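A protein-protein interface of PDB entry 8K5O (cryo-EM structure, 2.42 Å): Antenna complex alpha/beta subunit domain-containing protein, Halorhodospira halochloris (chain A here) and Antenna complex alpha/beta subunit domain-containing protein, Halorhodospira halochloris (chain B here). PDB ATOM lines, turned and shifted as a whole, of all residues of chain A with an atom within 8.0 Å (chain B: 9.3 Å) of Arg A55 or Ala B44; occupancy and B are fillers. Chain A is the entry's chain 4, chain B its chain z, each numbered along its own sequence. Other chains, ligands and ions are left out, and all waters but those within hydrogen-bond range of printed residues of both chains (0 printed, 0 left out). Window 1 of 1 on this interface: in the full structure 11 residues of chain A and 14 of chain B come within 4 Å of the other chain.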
ATOM      1  N   PRO A  49     -10.156   6.813   5.857  1.00  0.00           N
ATOM      2  CA  PRO A  49     -11.253   7.636   5.334  1.00  0.00           C
ATOM      3  C   PRO A  49     -10.862   9.095   5.213  1.00  0.00           C
ATOM      4  O   PRO A  49     -10.177   9.646   6.086  1.00  0.00           O
ATOM      5  CB  PRO A  49     -12.374   7.439   6.366  1.00  0.00           C
ATOM      6  CG  PRO A  49     -11.981   6.265   7.178  1.00  0.00           C
ATOM      7  CD  PRO A  49     -10.504   6.137   7.115  1.00  0.00           C
ATOM      8  N   PRO A  50     -11.289   9.756   4.139  1.00  0.00           N
ATOM      9  CA  PRO A  50     -11.121  11.210   4.043  1.00  0.00           C
ATOM     10  C   PRO A  50     -12.142  11.943   4.897  1.00  0.00           C
ATOM     11  O   PRO A  50     -12.949  11.304   5.577  1.00  0.00           O
ATOM     12  CB  PRO A  50     -11.329  11.485   2.551  1.00  0.00           C
ATOM     13  CG  PRO A  50     -12.204  10.370   2.093  1.00  0.00           C
ATOM     14  CD  PRO A  50     -11.842   9.173   2.907  1.00  0.00           C
ATOM     15  N   GLU A  51     -12.124  13.277   4.868  1.00  0.00           N
ATOM     16  CA  GLU A  51     -13.079  14.043   5.662  1.00  0.00           C
ATOM     17  C   GLU A  51     -14.514  13.682   5.305  1.00  0.00           C
ATOM     18  O   GLU A  51     -15.367  13.585   6.193  1.00  0.00           O
ATOM     19  CB  GLU A  51     -12.857  15.542   5.461  1.00  0.00           C
ATOM     20  CG  GLU A  51     -11.516  16.059   5.951  1.00  0.00           C
ATOM     21  CD  GLU A  51     -11.375  16.005   7.456  1.00  0.00           C
ATOM     22  OE1 GLU A  51     -12.397  16.150   8.157  1.00  0.00           O
ATOM     23  OE2 GLU A  51     -10.238  15.826   7.941  1.00  0.00           O
ATOM     24  N   GLN A  52     -14.793  13.471   4.018  1.00  0.00           N
ATOM     25  CA  GLN A  52     -16.122  13.099   3.554  1.00  0.00           C
ATOM     26  C   GLN A  52     -16.434  11.634   3.790  1.00  0.00           C
ATOM     27  O   GLN A  52     -17.569  11.210   3.553  1.00  0.00           O
ATOM     28  CB  GLN A  52     -16.262  13.399   2.064  1.00  0.00           C
ATOM     29  CG  GLN A  52     -15.500  12.442   1.178  1.00  0.00           C
ATOM     30  CD  GLN A  52     -14.133  12.959   0.810  1.00  0.00           C
ATOM     31  OE1 GLN A  52     -13.594  13.843   1.472  1.00  0.00           O
ATOM     32  NE2 GLN A  52     -13.555  12.402  -0.245  1.00  0.00           N
ATOM     33  N   GLY A  53     -15.459  10.859   4.235  1.00  0.00           N
ATOM     34  CA  GLY A  53     -15.645   9.439   4.406  1.00  0.00           C
ATOM     35  C   GLY A  53     -15.698   8.727   3.070  1.00  0.00           C
ATOM     36  O   GLY A  53     -15.556   9.306   1.997  1.00  0.00           O
ATOM     37  N   TYR A  54     -15.871   7.412   3.212  1.00  0.00           N
ATOM     38  CA  TYR A  54     -16.064   6.524   2.042  1.00  0.00           C
ATOM     39  C   TYR A  54     -17.194   5.511   2.290  1.00  0.00           C
ATOM     40  O   TYR A  54     -17.111   4.407   1.769  1.00  0.00           O
ATOM     41  CB  TYR A  54     -14.768   5.862   1.569  1.00  0.00           C
ATOM     42  CG  TYR A  54     -13.848   5.187   2.541  1.00  0.00           C
ATOM     43  CD1 TYR A  54     -14.288   4.188   3.383  1.00  0.00           C
ATOM     44  CD2 TYR A  54     -12.500   5.478   2.517  1.00  0.00           C
ATOM     45  CE1 TYR A  54     -13.421   3.541   4.238  1.00  0.00           C
ATOM     46  CE2 TYR A  54     -11.620   4.840   3.363  1.00  0.00           C
ATOM     47  CZ  TYR A  54     -12.087   3.883   4.236  1.00  0.00           C
ATOM     48  OH  TYR A  54     -11.231   3.253   5.069  1.00  0.00           O
ATOM     49  N   ARG A  55     -18.196   5.830   3.104  1.00  0.00           N
ATOM     50  CA  ARG A  55     -19.357   4.962   3.188  1.00  0.00           C
ATOM     51  C   ARG A  55     -20.091   4.986   1.855  1.00  0.00           C
ATOM     52  O   ARG A  55     -20.381   6.056   1.316  1.00  0.00           O
ATOM     53  CB  ARG A  55     -20.272   5.418   4.314  1.00  0.00           C
ATOM     54  CG  ARG A  55     -19.831   4.967   5.674  1.00  0.00           C
ATOM     55  CD  ARG A  55     -20.938   5.152   6.677  1.00  0.00           C
ATOM     56  NE  ARG A  55     -21.553   6.465   6.542  1.00  0.00           N
ATOM     57  CZ  ARG A  55     -22.377   6.999   7.430  1.00  0.00           C
ATOM     58  NH1 ARG A  55     -22.685   6.369   8.550  1.00  0.00           N
ATOM     59  NH2 ARG A  55     -22.897   8.199   7.194  1.00  0.00           N
ATOM     60  N   LEU A  56     -20.385   3.800   1.319  1.00  0.00           N
ATOM     61  CA  LEU A  56     -21.031   3.724   0.014  1.00  0.00           C
ATOM     62  C   LEU A  56     -22.409   4.371   0.028  1.00  0.00           C
ATOM     63  O   LEU A  56     -22.841   4.932  -0.984  1.00  0.00           O
ATOM     64  CB  LEU A  56     -21.125   2.265  -0.434  1.00  0.00           C
ATOM     65  CG  LEU A  56     -21.494   2.024  -1.897  1.00  0.00           C
ATOM     66  CD1 LEU A  56     -20.450   2.598  -2.837  1.00  0.00           C
ATOM     67  CD2 LEU A  56     -21.698   0.547  -2.152  1.00  0.00           C
ATOM     68  N   GLU A  57     -23.104   4.314   1.163  1.00  0.00           N
ATOM     69  CA  GLU A  57     -24.418   4.937   1.273  1.00  0.00           C
ATOM     70  C   GLU A  57     -24.350   6.449   1.111  1.00  0.00           C
ATOM     71  O   GLU A  57     -25.347   7.078   0.744  1.00  0.00           O
ATOM     72  CB  GLU A  57     -25.042   4.569   2.615  1.00  0.00           C
ATOM     73  CG  GLU A  57     -24.253   5.062   3.811  1.00  0.00           C
ATOM     74  CD  GLU A  57     -24.853   4.609   5.119  1.00  0.00           C
ATOM     75  OE1 GLU A  57     -25.878   3.900   5.089  1.00  0.00           O
ATOM     76  OE2 GLU A  57     -24.304   4.962   6.181  1.00  0.00           O
ATOM     77  N   ASP A  58     -23.193   7.051   1.378  1.00  0.00           N
ATOM     78  CA  ASP A  58     -23.059   8.497   1.279  1.00  0.00           C
ATOM     79  C   ASP A  58     -22.816   8.983  -0.142  1.00  0.00           C
ATOM     80  O   ASP A  58     -22.888  10.192  -0.383  1.00  0.00           O
ATOM     81  CB  ASP A  58     -21.926   8.980   2.183  1.00  0.00           C
ATOM     82  CG  ASP A  58     -22.292   8.931   3.649  1.00  0.00           C
ATOM     83  OD1 ASP A  58     -23.367   9.448   4.012  1.00  0.00           O
ATOM     84  OD2 ASP A  58     -21.504   8.379   4.442  1.00  0.00           O
ATOM     85  N   PHE A  59     -22.541   8.084  -1.084  1.00  0.00           N
ATOM     86  CA  PHE A  59     -22.177   8.503  -2.431  1.00  0.00           C
ATOM     87  C   PHE A  59     -23.017   7.798  -3.484  1.00  0.00           C
ATOM     88  O   PHE A  59     -23.300   8.366  -4.542  1.00  0.00           O
ATOM     89  CB  PHE A  59     -20.693   8.241  -2.678  1.00  0.00           C
ATOM     90  CG  PHE A  59     -19.785   9.000  -1.758  1.00  0.00           C
ATOM     91  CD1 PHE A  59     -19.456   8.492  -0.514  1.00  0.00           C
ATOM     92  CD2 PHE A  59     -19.269  10.223  -2.131  1.00  0.00           C
ATOM     93  CE1 PHE A  59     -18.627   9.186   0.333  1.00  0.00           C
ATOM     94  CE2 PHE A  59     -18.441  10.921  -1.285  1.00  0.00           C
ATOM     95  CZ  PHE A  59     -18.121  10.402  -0.052  1.00  0.00           C
ATOM     96  N   ALA A  60     -23.415   6.568  -3.209  1.00  0.00           N
ATOM     97  CA  ALA A  60     -24.160   5.800  -4.189  1.00  0.00           C
ATOM     98  C   ALA A  60     -25.638   6.176  -4.159  1.00  0.00           C
ATOM     99  O   ALA A  60     -26.161   6.589  -3.121  1.00  0.00           O
ATOM    100  CB  ALA A  60     -24.002   4.308  -3.926  1.00  0.00           C
ATOM    101  N   THR A  66     -26.435  -0.721  -0.041  1.00  0.00           N
ATOM    102  CA  THR A  66     -25.330  -0.479   0.872  1.00  0.00           C
ATOM    103  C   THR A  66     -25.693  -1.051   2.231  1.00  0.00           C
ATOM    104  O   THR A  66     -26.769  -0.765   2.762  1.00  0.00           O
ATOM    105  CB  THR A  66     -25.026   1.016   0.990  1.00  0.00           C
ATOM    106  OG1 THR A  66     -26.065   1.656   1.739  1.00  0.00           O
ATOM    107  CG2 THR A  66     -24.929   1.655  -0.384  1.00  0.00           C
ATOM    108  N   ASP A  67     -24.803  -1.865   2.784  1.00  0.00           N
ATOM    109  CA  ASP A  67     -25.012  -2.492   4.079  1.00  0.00           C
ATOM    110  C   ASP A  67     -24.013  -1.910   5.067  1.00  0.00           C
ATOM    111  O   ASP A  67     -22.807  -1.906   4.805  1.00  0.00           O
ATOM    112  CB  ASP A  67     -24.851  -4.011   3.982  1.00  0.00           C
ATOM    113  CG  ASP A  67     -25.385  -4.736   5.199  1.00  0.00           C
ATOM    114  OD1 ASP A  67     -25.883  -4.066   6.127  1.00  0.00           O
ATOM    115  OD2 ASP A  67     -25.303  -5.983   5.228  1.00  0.00           O
ATOM    116  N   SER A  68     -24.515  -1.411   6.191  1.00  0.00           N
ATOM    117  CA  SER A  68     -23.649  -0.808   7.191  1.00  0.00           C
ATOM    118  C   SER A  68     -22.737  -1.854   7.818  1.00  0.00           C
ATOM    119  O   SER A  68     -23.070  -3.041   7.892  1.00  0.00           O
ATOM    120  CB  SER A  68     -24.482  -0.127   8.273  1.00  0.00           C
ATOM    121  OG  SER A  68     -25.235  -1.078   9.002  1.00  0.00           O
ATOM    122  N   PHE A  69     -21.565  -1.401   8.266  1.00  0.00           N
ATOM    123  CA  PHE A  69     -20.647  -2.296   8.959  1.00  0.00           C
ATOM    124  C   PHE A  69     -21.279  -2.844  10.229  1.00  0.00           C
ATOM    125  O   PHE A  69     -21.153  -4.035  10.532  1.00  0.00           O
ATOM    126  CB  PHE A  69     -19.343  -1.562   9.281  1.00  0.00           C
ATOM    127  CG  PHE A  69     -18.374  -2.370  10.089  1.00  0.00           C
ATOM    128  CD1 PHE A  69     -17.489  -3.233   9.470  1.00  0.00           C
ATOM    129  CD2 PHE A  69     -18.336  -2.253  11.467  1.00  0.00           C
ATOM    130  CE1 PHE A  69     -16.595  -3.974  10.213  1.00  0.00           C
ATOM    131  CE2 PHE A  69     -17.450  -2.993  12.210  1.00  0.00           C
ATOM    132  CZ  PHE A  69     -16.576  -3.852  11.584  1.00  0.00           C
ATOM    133  N   TYR A  70     -22.008  -2.008  10.931  1.00  0.00           N
ATOM    134  CA  TYR A  70     -22.619  -2.445  12.128  1.00  0.00           C
ATOM    135  C   TYR A  70     -23.905  -3.154  11.840  1.00  0.00           C
ATOM    136  O   TYR A  70     -24.684  -2.697  11.038  1.00  0.00           O
ATOM    137  CB  TYR A  70     -22.845  -1.259  13.058  1.00  0.00           C
ATOM    138  CG  TYR A  70     -21.628  -0.478  13.404  1.00  0.00           C
ATOM    139  CD1 TYR A  70     -20.527  -1.085  13.976  1.00  0.00           C
ATOM    140  CD2 TYR A  70     -21.588   0.871  13.173  1.00  0.00           C
ATOM    141  CE1 TYR A  70     -19.413  -0.359  14.302  1.00  0.00           C
ATOM    142  CE2 TYR A  70     -20.479   1.606  13.485  1.00  0.00           C
ATOM    143  CZ  TYR A  70     -19.403   0.990  14.050  1.00  0.00           C
ATOM    144  OH  TYR A  70     -18.329   1.754  14.344  1.00  0.00           O
ATOM    145  N   CYS B  32     -11.689   1.894  18.162  1.00  0.00           N
ATOM    146  CA  CYS B  32     -11.844   2.721  16.971  1.00  0.00           C
ATOM    147  C   CYS B  32     -12.928   2.166  16.063  1.00  0.00           C
ATOM    148  O   CYS B  32     -13.752   2.920  15.537  1.00  0.00           O
ATOM    149  CB  CYS B  32     -10.524   2.814  16.214  1.00  0.00           C
ATOM    150  SG  CYS B  32      -9.114   3.211  17.227  1.00  0.00           S
ATOM    151  N   ILE B  33     -12.944   0.846  15.869  1.00  0.00           N
ATOM    152  CA  ILE B  33     -13.977   0.224  15.047  1.00  0.00           C
ATOM    153  C   ILE B  33     -15.360   0.498  15.625  1.00  0.00           C
ATOM    154  O   ILE B  33     -16.326   0.731  14.888  1.00  0.00           O
ATOM    155  CB  ILE B  33     -13.709  -1.286  14.911  1.00  0.00           C
ATOM    156  CG1 ILE B  33     -12.442  -1.529  14.101  1.00  0.00           C
ATOM    157  CG2 ILE B  33     -14.882  -1.983  14.265  1.00  0.00           C
ATOM    158  CD1 ILE B  33     -11.846  -2.899  14.305  1.00  0.00           C
ATOM    159  N   SER B  35     -16.267   3.088  17.229  1.00  0.00           N
ATOM    160  CA  SER B  35     -16.602   4.491  17.048  1.00  0.00           C
ATOM    161  C   SER B  35     -16.955   4.760  15.593  1.00  0.00           C
ATOM    162  O   SER B  35     -16.219   4.362  14.687  1.00  0.00           O
ATOM    163  CB  SER B  35     -15.434   5.374  17.477  1.00  0.00           C
ATOM    164  OG  SER B  35     -15.677   6.726  17.148  1.00  0.00           O
ATOM    165  N   GLU B  36     -18.082   5.434  15.368  1.00  0.00           N
ATOM    166  CA  GLU B  36     -18.446   5.818  14.009  1.00  0.00           C
ATOM    167  C   GLU B  36     -17.396   6.733  13.401  1.00  0.00           C
ATOM    168  O   GLU B  36     -17.013   6.570  12.239  1.00  0.00           O
ATOM    169  CB  GLU B  36     -19.804   6.511  14.004  1.00  0.00           C
ATOM    170  CG  GLU B  36     -20.252   6.925  12.622  1.00  0.00           C
ATOM    171  CD  GLU B  36     -21.539   7.705  12.635  1.00  0.00           C
ATOM    172  OE1 GLU B  36     -22.058   7.983  13.734  1.00  0.00           O
ATOM    173  OE2 GLU B  36     -22.040   8.032  11.543  1.00  0.00           O
ATOM    174  N   ARG B  37     -16.923   7.706  14.178  1.00  0.00           N
ATOM    175  CA  ARG B  37     -15.943   8.658  13.674  1.00  0.00           C
ATOM    176  C   ARG B  37     -14.622   7.978  13.356  1.00  0.00           C
ATOM    177  O   ARG B  37     -13.907   8.388  12.436  1.00  0.00           O
ATOM    178  CB  ARG B  37     -15.742   9.771  14.699  1.00  0.00           C
ATOM    179  CG  ARG B  37     -14.619  10.720  14.388  1.00  0.00           C
ATOM    180  CD  ARG B  37     -14.501  11.758  15.469  1.00  0.00           C
ATOM    181  NE  ARG B  37     -13.347  12.626  15.286  1.00  0.00           N
ATOM    182  CZ  ARG B  37     -13.307  13.641  14.436  1.00  0.00           C
ATOM    183  NH1 ARG B  37     -14.329  13.918  13.644  1.00  0.00           N
ATOM    184  NH2 ARG B  37     -12.219  14.398  14.380  1.00  0.00           N
ATOM    185  N   PHE B  38     -14.287   6.930  14.095  1.00  0.00           N
ATOM    186  CA  PHE B  38     -12.969   6.325  14.026  1.00  0.00           C
ATOM    187  C   PHE B  38     -12.967   4.945  13.390  1.00  0.00           C
ATOM    188  O   PHE B  38     -11.896   4.349  13.251  1.00  0.00           O
ATOM    189  CB  PHE B  38     -12.377   6.254  15.430  1.00  0.00           C
ATOM    190  CG  PHE B  38     -12.296   7.585  16.109  1.00  0.00           C
ATOM    191  CD1 PHE B  38     -11.758   8.677  15.452  1.00  0.00           C
ATOM    192  CD2 PHE B  38     -12.746   7.747  17.405  1.00  0.00           C
ATOM    193  CE1 PHE B  38     -11.667   9.893  16.078  1.00  0.00           C
ATOM    194  CE2 PHE B  38     -12.663   8.968  18.028  1.00  0.00           C
ATOM    195  CZ  PHE B  38     -12.125  10.039  17.364  1.00  0.00           C
ATOM    196  N   ASN B  39     -14.125   4.422  12.999  1.00  0.00           N
ATOM    197  CA  ASN B  39     -14.184   3.137  12.306  1.00  0.00           C
ATOM    198  C   ASN B  39     -13.697   3.362  10.888  1.00  0.00           C
ATOM    199  O   ASN B  39     -14.462   3.709   9.989  1.00  0.00           O
ATOM    200  CB  ASN B  39     -15.595   2.565  12.327  1.00  0.00           C
ATOM    201  CG  ASN B  39     -15.648   1.131  11.857  1.00  0.00           C
ATOM    202  OD1 ASN B  39     -14.620   0.482  11.692  1.00  0.00           O
ATOM    203  ND2 ASN B  39     -16.850   0.630  11.632  1.00  0.00           N
ATOM    204  N   TRP B  40     -12.395   3.177  10.691  1.00  0.00           N
ATOM    205  CA  TRP B  40     -11.815   3.324   9.366  1.00  0.00           C
ATOM    206  C   TRP B  40     -12.307   2.252   8.406  1.00  0.00           C
ATOM    207  O   TRP B  40     -12.257   2.461   7.194  1.00  0.00           O
ATOM    208  CB  TRP B  40     -10.289   3.297   9.459  1.00  0.00           C
ATOM    209  CG  TRP B  40      -9.715   1.951   9.781  1.00  0.00           C
ATOM    210  CD1 TRP B  40      -9.122   1.090   8.912  1.00  0.00           C
ATOM    211  CD2 TRP B  40      -9.678   1.314  11.064  1.00  0.00           C
ATOM    212  NE1 TRP B  40      -8.715  -0.040   9.569  1.00  0.00           N
ATOM    213  CE2 TRP B  40      -9.046   0.070  10.893  1.00  0.00           C
ATOM    214  CE3 TRP B  40     -10.115   1.675  12.340  1.00  0.00           C
ATOM    215  CZ2 TRP B  40      -8.840  -0.814  11.946  1.00  0.00           C
ATOM    216  CZ3 TRP B  40      -9.909   0.799  13.381  1.00  0.00           C
ATOM    217  CH2 TRP B  40      -9.277  -0.431  13.180  1.00  0.00           C
ATOM    218  N   LEU B  41     -12.792   1.122   8.918  1.00  0.00           N
ATOM    219  CA  LEU B  41     -13.283   0.061   8.047  1.00  0.00           C
ATOM    220  C   LEU B  41     -14.558   0.479   7.329  1.00  0.00           C
ATOM    221  O   LEU B  41     -14.696   0.274   6.119  1.00  0.00           O
ATOM    222  CB  LEU B  41     -13.517  -1.210   8.856  1.00  0.00           C
ATOM    223  CG  LEU B  41     -12.381  -1.669   9.762  1.00  0.00           C
ATOM    224  CD1 LEU B  41     -12.908  -2.680  10.753  1.00  0.00           C
ATOM    225  CD2 LEU B  41     -11.254  -2.256   8.941  1.00  0.00           C
ATOM    226  N   GLU B  42     -15.515   1.046   8.068  1.00  0.00           N
ATOM    227  CA  GLU B  42     -16.738   1.537   7.442  1.00  0.00           C
ATOM    228  C   GLU B  42     -16.495   2.859   6.726  1.00  0.00           C
ATOM    229  O   GLU B  42     -17.093   3.122   5.678  1.00  0.00           O
ATOM    230  CB  GLU B  42     -17.843   1.668   8.489  1.00  0.00           C
ATOM    231  CG  GLU B  42     -19.165   2.236   7.980  1.00  0.00           C
ATOM    232  CD  GLU B  42     -19.824   1.381   6.902  1.00  0.00           C
ATOM    233  OE1 GLU B  42     -19.509   0.182   6.794  1.00  0.00           O
ATOM    234  OE2 GLU B  42     -20.678   1.911   6.162  1.00  0.00           O
ATOM    235  N   GLY B  43     -15.602   3.685   7.258  1.00  0.00           N
ATOM    236  CA  GLY B  43     -15.281   4.958   6.640  1.00  0.00           C
ATOM    237  C   GLY B  43     -16.392   5.981   6.666  1.00  0.00           C
ATOM    238  O   GLY B  43     -16.652   6.633   5.649  1.00  0.00           O
ATOM    239  N   ALA B  44     -17.056   6.140   7.805  1.00  0.00           N
ATOM    240  CA  ALA B  44     -18.069   7.170   7.935  1.00  0.00           C
ATOM    241  C   ALA B  44     -17.423   8.548   7.833  1.00  0.00           C
ATOM    242  O   ALA B  44     -16.254   8.721   8.184  1.00  0.00           O
ATOM    243  CB  ALA B  44     -18.806   7.031   9.263  1.00  0.00           C
ATOM    244  N   PRO B  45     -18.154   9.545   7.337  1.00  0.00           N
ATOM    245  CA  PRO B  45     -17.588  10.894   7.261  1.00  0.00           C
ATOM    246  C   PRO B  45     -17.318  11.461   8.643  1.00  0.00           C
ATOM    247  O   PRO B  45     -17.992  11.131   9.621  1.00  0.00           O
ATOM    248  CB  PRO B  45     -18.672  11.693   6.530  1.00  0.00           C
ATOM    249  CG  PRO B  45     -19.913  10.906   6.705  1.00  0.00           C
ATOM    250  CD  PRO B  45     -19.500   9.479   6.750  1.00  0.00           C
ATOM    251  N   ALA B  46     -16.302  12.308   8.719  1.00  0.00           N
ATOM    252  CA  ALA B  46     -16.062  13.076   9.927  1.00  0.00           C
ATOM    253  C   ALA B  46     -16.969  14.297   9.945  1.00  0.00           C
ATOM    254  O   ALA B  46     -17.301  14.865   8.902  1.00  0.00           O
ATOM    255  CB  ALA B  46     -14.598  13.505  10.015  1.00  0.00           C
ATOM    256  N   ALA B  47     -17.374  14.702  11.149  1.00  0.00           N
ATOM    257  CA  ALA B  47     -18.202  15.893  11.280  1.00  0.00           C
ATOM    258  C   ALA B  47     -17.486  17.142  10.794  1.00  0.00           C
ATOM    259  O   ALA B  47     -18.146  18.136  10.480  1.00  0.00           O
ATOM    260  CB  ALA B  47     -18.642  16.076  12.728  1.00  0.00           C
ATOM    261  N   GLU B  48     -16.152  17.112  10.726  1.00  0.00           N
ATOM    262  CA  GLU B  48     -15.401  18.227  10.168  1.00  0.00           C
ATOM    263  C   GLU B  48     -15.701  18.445   8.694  1.00  0.00           C
ATOM    264  O   GLU B  48     -15.447  19.538   8.178  1.00  0.00           O
ATOM    265  CB  GLU B  48     -13.903  18.001  10.365  1.00  0.00           C
ATOM    266  CG  GLU B  48     -13.415  18.293  11.767  1.00  0.00           C
ATOM    267  CD  GLU B  48     -13.361  17.055  12.636  1.00  0.00           C
ATOM    268  OE1 GLU B  48     -14.074  16.078  12.328  1.00  0.00           O
ATOM    269  OE2 GLU B  48     -12.609  17.063  13.632  1.00  0.00           O
ATOM    270  N   TYR B  49     -16.223  17.432   8.001  1.00  0.00           N
ATOM    271  CA  TYR B  49     -16.624  17.621   6.613  1.00  0.00           C
ATOM    272  C   TYR B  49     -17.749  18.635   6.493  1.00  0.00           C
ATOM    273  O   TYR B  49     -17.791  19.409   5.532  1.00  0.00           O
ATOM    274  CB  TYR B  49     -17.067  16.295   5.996  1.00  0.00           C
ATOM    275  CG  TYR B  49     -17.209  16.369   4.498  1.00  0.00           C
ATOM    276  CD1 TYR B  49     -16.246  16.999   3.726  1.00  0.00           C
ATOM    277  CD2 TYR B  49     -18.327  15.856   3.859  1.00  0.00           C
ATOM    278  CE1 TYR B  49     -16.374  17.088   2.363  1.00  0.00           C
ATOM    279  CE2 TYR B  49     -18.467  15.944   2.495  1.00  0.00           C
ATOM    280  CZ  TYR B  49     -17.485  16.560   1.750  1.00  0.00           C
ATOM    281  OH  TYR B  49     -17.613  16.649   0.386  1.00  0.00           O
ATOM    282  N   TYR B  50     -18.667  18.643   7.455  1.00  0.00           N
ATOM    283  CA  TYR B  50     -19.884  19.428   7.372  1.00  0.00           C
ATOM    284  C   TYR B  50     -19.842  20.702   8.198  1.00  0.00           C
ATOM    285  O   TYR B  50     -20.858  21.398   8.282  1.00  0.00           O
ATOM    286  CB  TYR B  50     -21.074  18.569   7.799  1.00  0.00           C
ATOM    287  CG  TYR B  50     -21.190  17.295   7.003  1.00  0.00           C
ATOM    288  CD1 TYR B  50     -21.678  17.311   5.706  1.00  0.00           C
ATOM    289  CD2 TYR B  50     -20.800  16.077   7.542  1.00  0.00           C
ATOM    290  CE1 TYR B  50     -21.784  16.154   4.972  1.00  0.00           C
ATOM    291  CE2 TYR B  50     -20.903  14.914   6.813  1.00  0.00           C
ATOM    292  CZ  TYR B  50     -21.397  14.958   5.529  1.00  0.00           C
ATOM    293  OH  TYR B  50     -21.504  13.804   4.792  1.00  0.00           O
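The guanidinium group (NE) of Arg A55 is in salt-bridge range of the side-chain carboxylate (OE2) of Glu A57 (3.2 Å). The side-chain hydroxyl (OG) of Ser A68 sits at hydrogen-bond distance from the backbone carbonyl oxygen (O) of Tyr A70 (2.7 Å). The backbone carbonyl oxygen (O) of Cys B32 is in hydrogen-bond range of the backbone NH (N) of Asn B39, 3.0 Å away. ND2 of Asn B39 sits close to O of Ile B33, at 3.3 Å. The side-chain hydroxyl of Ser B35 lies close to the backbone NH of Arg B37. The backbone NH (N) of Leu B41 lies close to the side-chain amide oxygen (OD1) of Asn B39 (3.4 Å).
O of Glu A51 sits at hydrogen-bond distance from N of Ala B46, 3.0 Å away. The backbone carbonyl oxygen (O) of Trp B40 sits at hydrogen-bond distance from the side-chain hydroxyl (OH) of Tyr A54 (2.5 Å). The backbone NH of Tyr A54 lies within hydrogen-bond range of the backbone carbonyl oxygen of Gly B43, 2.7 Å away. The guanidinium group of Arg A55 is in salt-bridge range of the side-chain carboxylate of Glu B36 (3.5 Å). The backbone NH (N) of Arg A55 lies within hydrogen-bond range of the backbone carbonyl oxygen (O) of Gly B43 (3.1 Å). The backbone NH of Phe A69 sits at hydrogen-bond distance from the side-chain carboxylate of Glu B42. OH of Tyr A70 is in hydrogen-bond range of O of Ser B35 (3.4 Å). The side-chain hydroxyl of Tyr A70 sits at hydrogen-bond distance from the side-chain amide nitrogen of Asn B39, at 3.3 Å. O of Ile B33 lies close to OH of Tyr A70, 2.3 Å away.
Arg A55 touches just these residues of chain B: Glu B36, Glu B42, Gly B43, Ala B44 and Pro B45. Of chain A, only Gly A53 and Arg A55 come within 4 Å of Ala B44. Of chain B, only Gly B43 (3.2 Å), Ala B44 (3.9 Å) and Pro B45 (3.7 Å) come within 4 Å of Gly A53. No residue of chain B comes within 4 Å of Glu A57. Asp A58 touches just one residue of chain B: Pro B45 (3.2 Å). Of chain A, only Pro A49 (3.6 Å), Gly A53 (3.2 Å), Tyr A54 (2.7 Å) and Arg A55 (3.1 Å) come within 4 Å of Gly B43. Of chain A, only Glu A51 (3.6 Å), Gln A52 (3.2 Å), Gly A53 (3.7 Å), Arg A55 (3.7 Å) and Asp A58 (3.2 Å) come within 4 Å of Pro B45. Of the printed residues of chain A, Ala B46 touches Glu A51 (3.0 Å). Printed residues of chain A within 4 Å of Ser B35: Tyr A70 (3.4 Å). Printed residues of chain A within 4 Å of Ile B33: Phe A69 and Tyr A70. Printed residues of chain A within 4 Å of Trp B40: Pro A49 and Tyr A54. Printed residues of chain B within 4 Å of Gln A52: Pro B45 (3.2 Å) and Tyr B49 (3.4 Å). Pro A50 touches none of the printed residues of chain B. The nearest residue of chain B that does not touch Arg A55 is Tyr B50 (6.3 Å).
Hydrophobic or aromatic side chains of chain B that line the printed part of chain A: Ile B33, Trp B40, Leu B41, Ala B44, Pro B45, Ala B46 and Tyr B49. Among the printed residues, 30 pairs touch across the chains.
Among the printed residues, merely in contact across the chains: Pro A49 with Trp B40 (3.7 Å), Pro A49 with Gly B43 (3.6 Å), Glu A51 with Pro B45 (3.6 Å), Glu A51 with Glu B48 (3.3 Å), Glu A51 with Tyr B49 (3.2 Å), Gln A52 with Pro B45 (3.2 Å), Gln A52 with Tyr B49 (3.4 Å), Gly A53 with Gly B43 (3.2 Å), Gly A53 with Ala B44 (3.9 Å), Gly A53 with Pro B45 (3.7 Å), Tyr A54 with Leu B41 (3.98 Å), Tyr A54 with Glu B42 (3.8 Å), Arg A55 with Glu B42 (3.2 Å), Arg A55 with Ala B44 (3.6 Å), Arg A55 with Pro B45 (3.7 Å), Asp A58 with Pro B45 (3.2 Å), Ser A68 with Glu B42 (3.95 Å), Phe A69 with Ile B33 (3.4 Å), Phe A69 with Asn B39 (3.2 Å), Phe A69 with Leu B41 (3.9 Å) and Tyr A70 with Glu B36 (3.8 Å).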
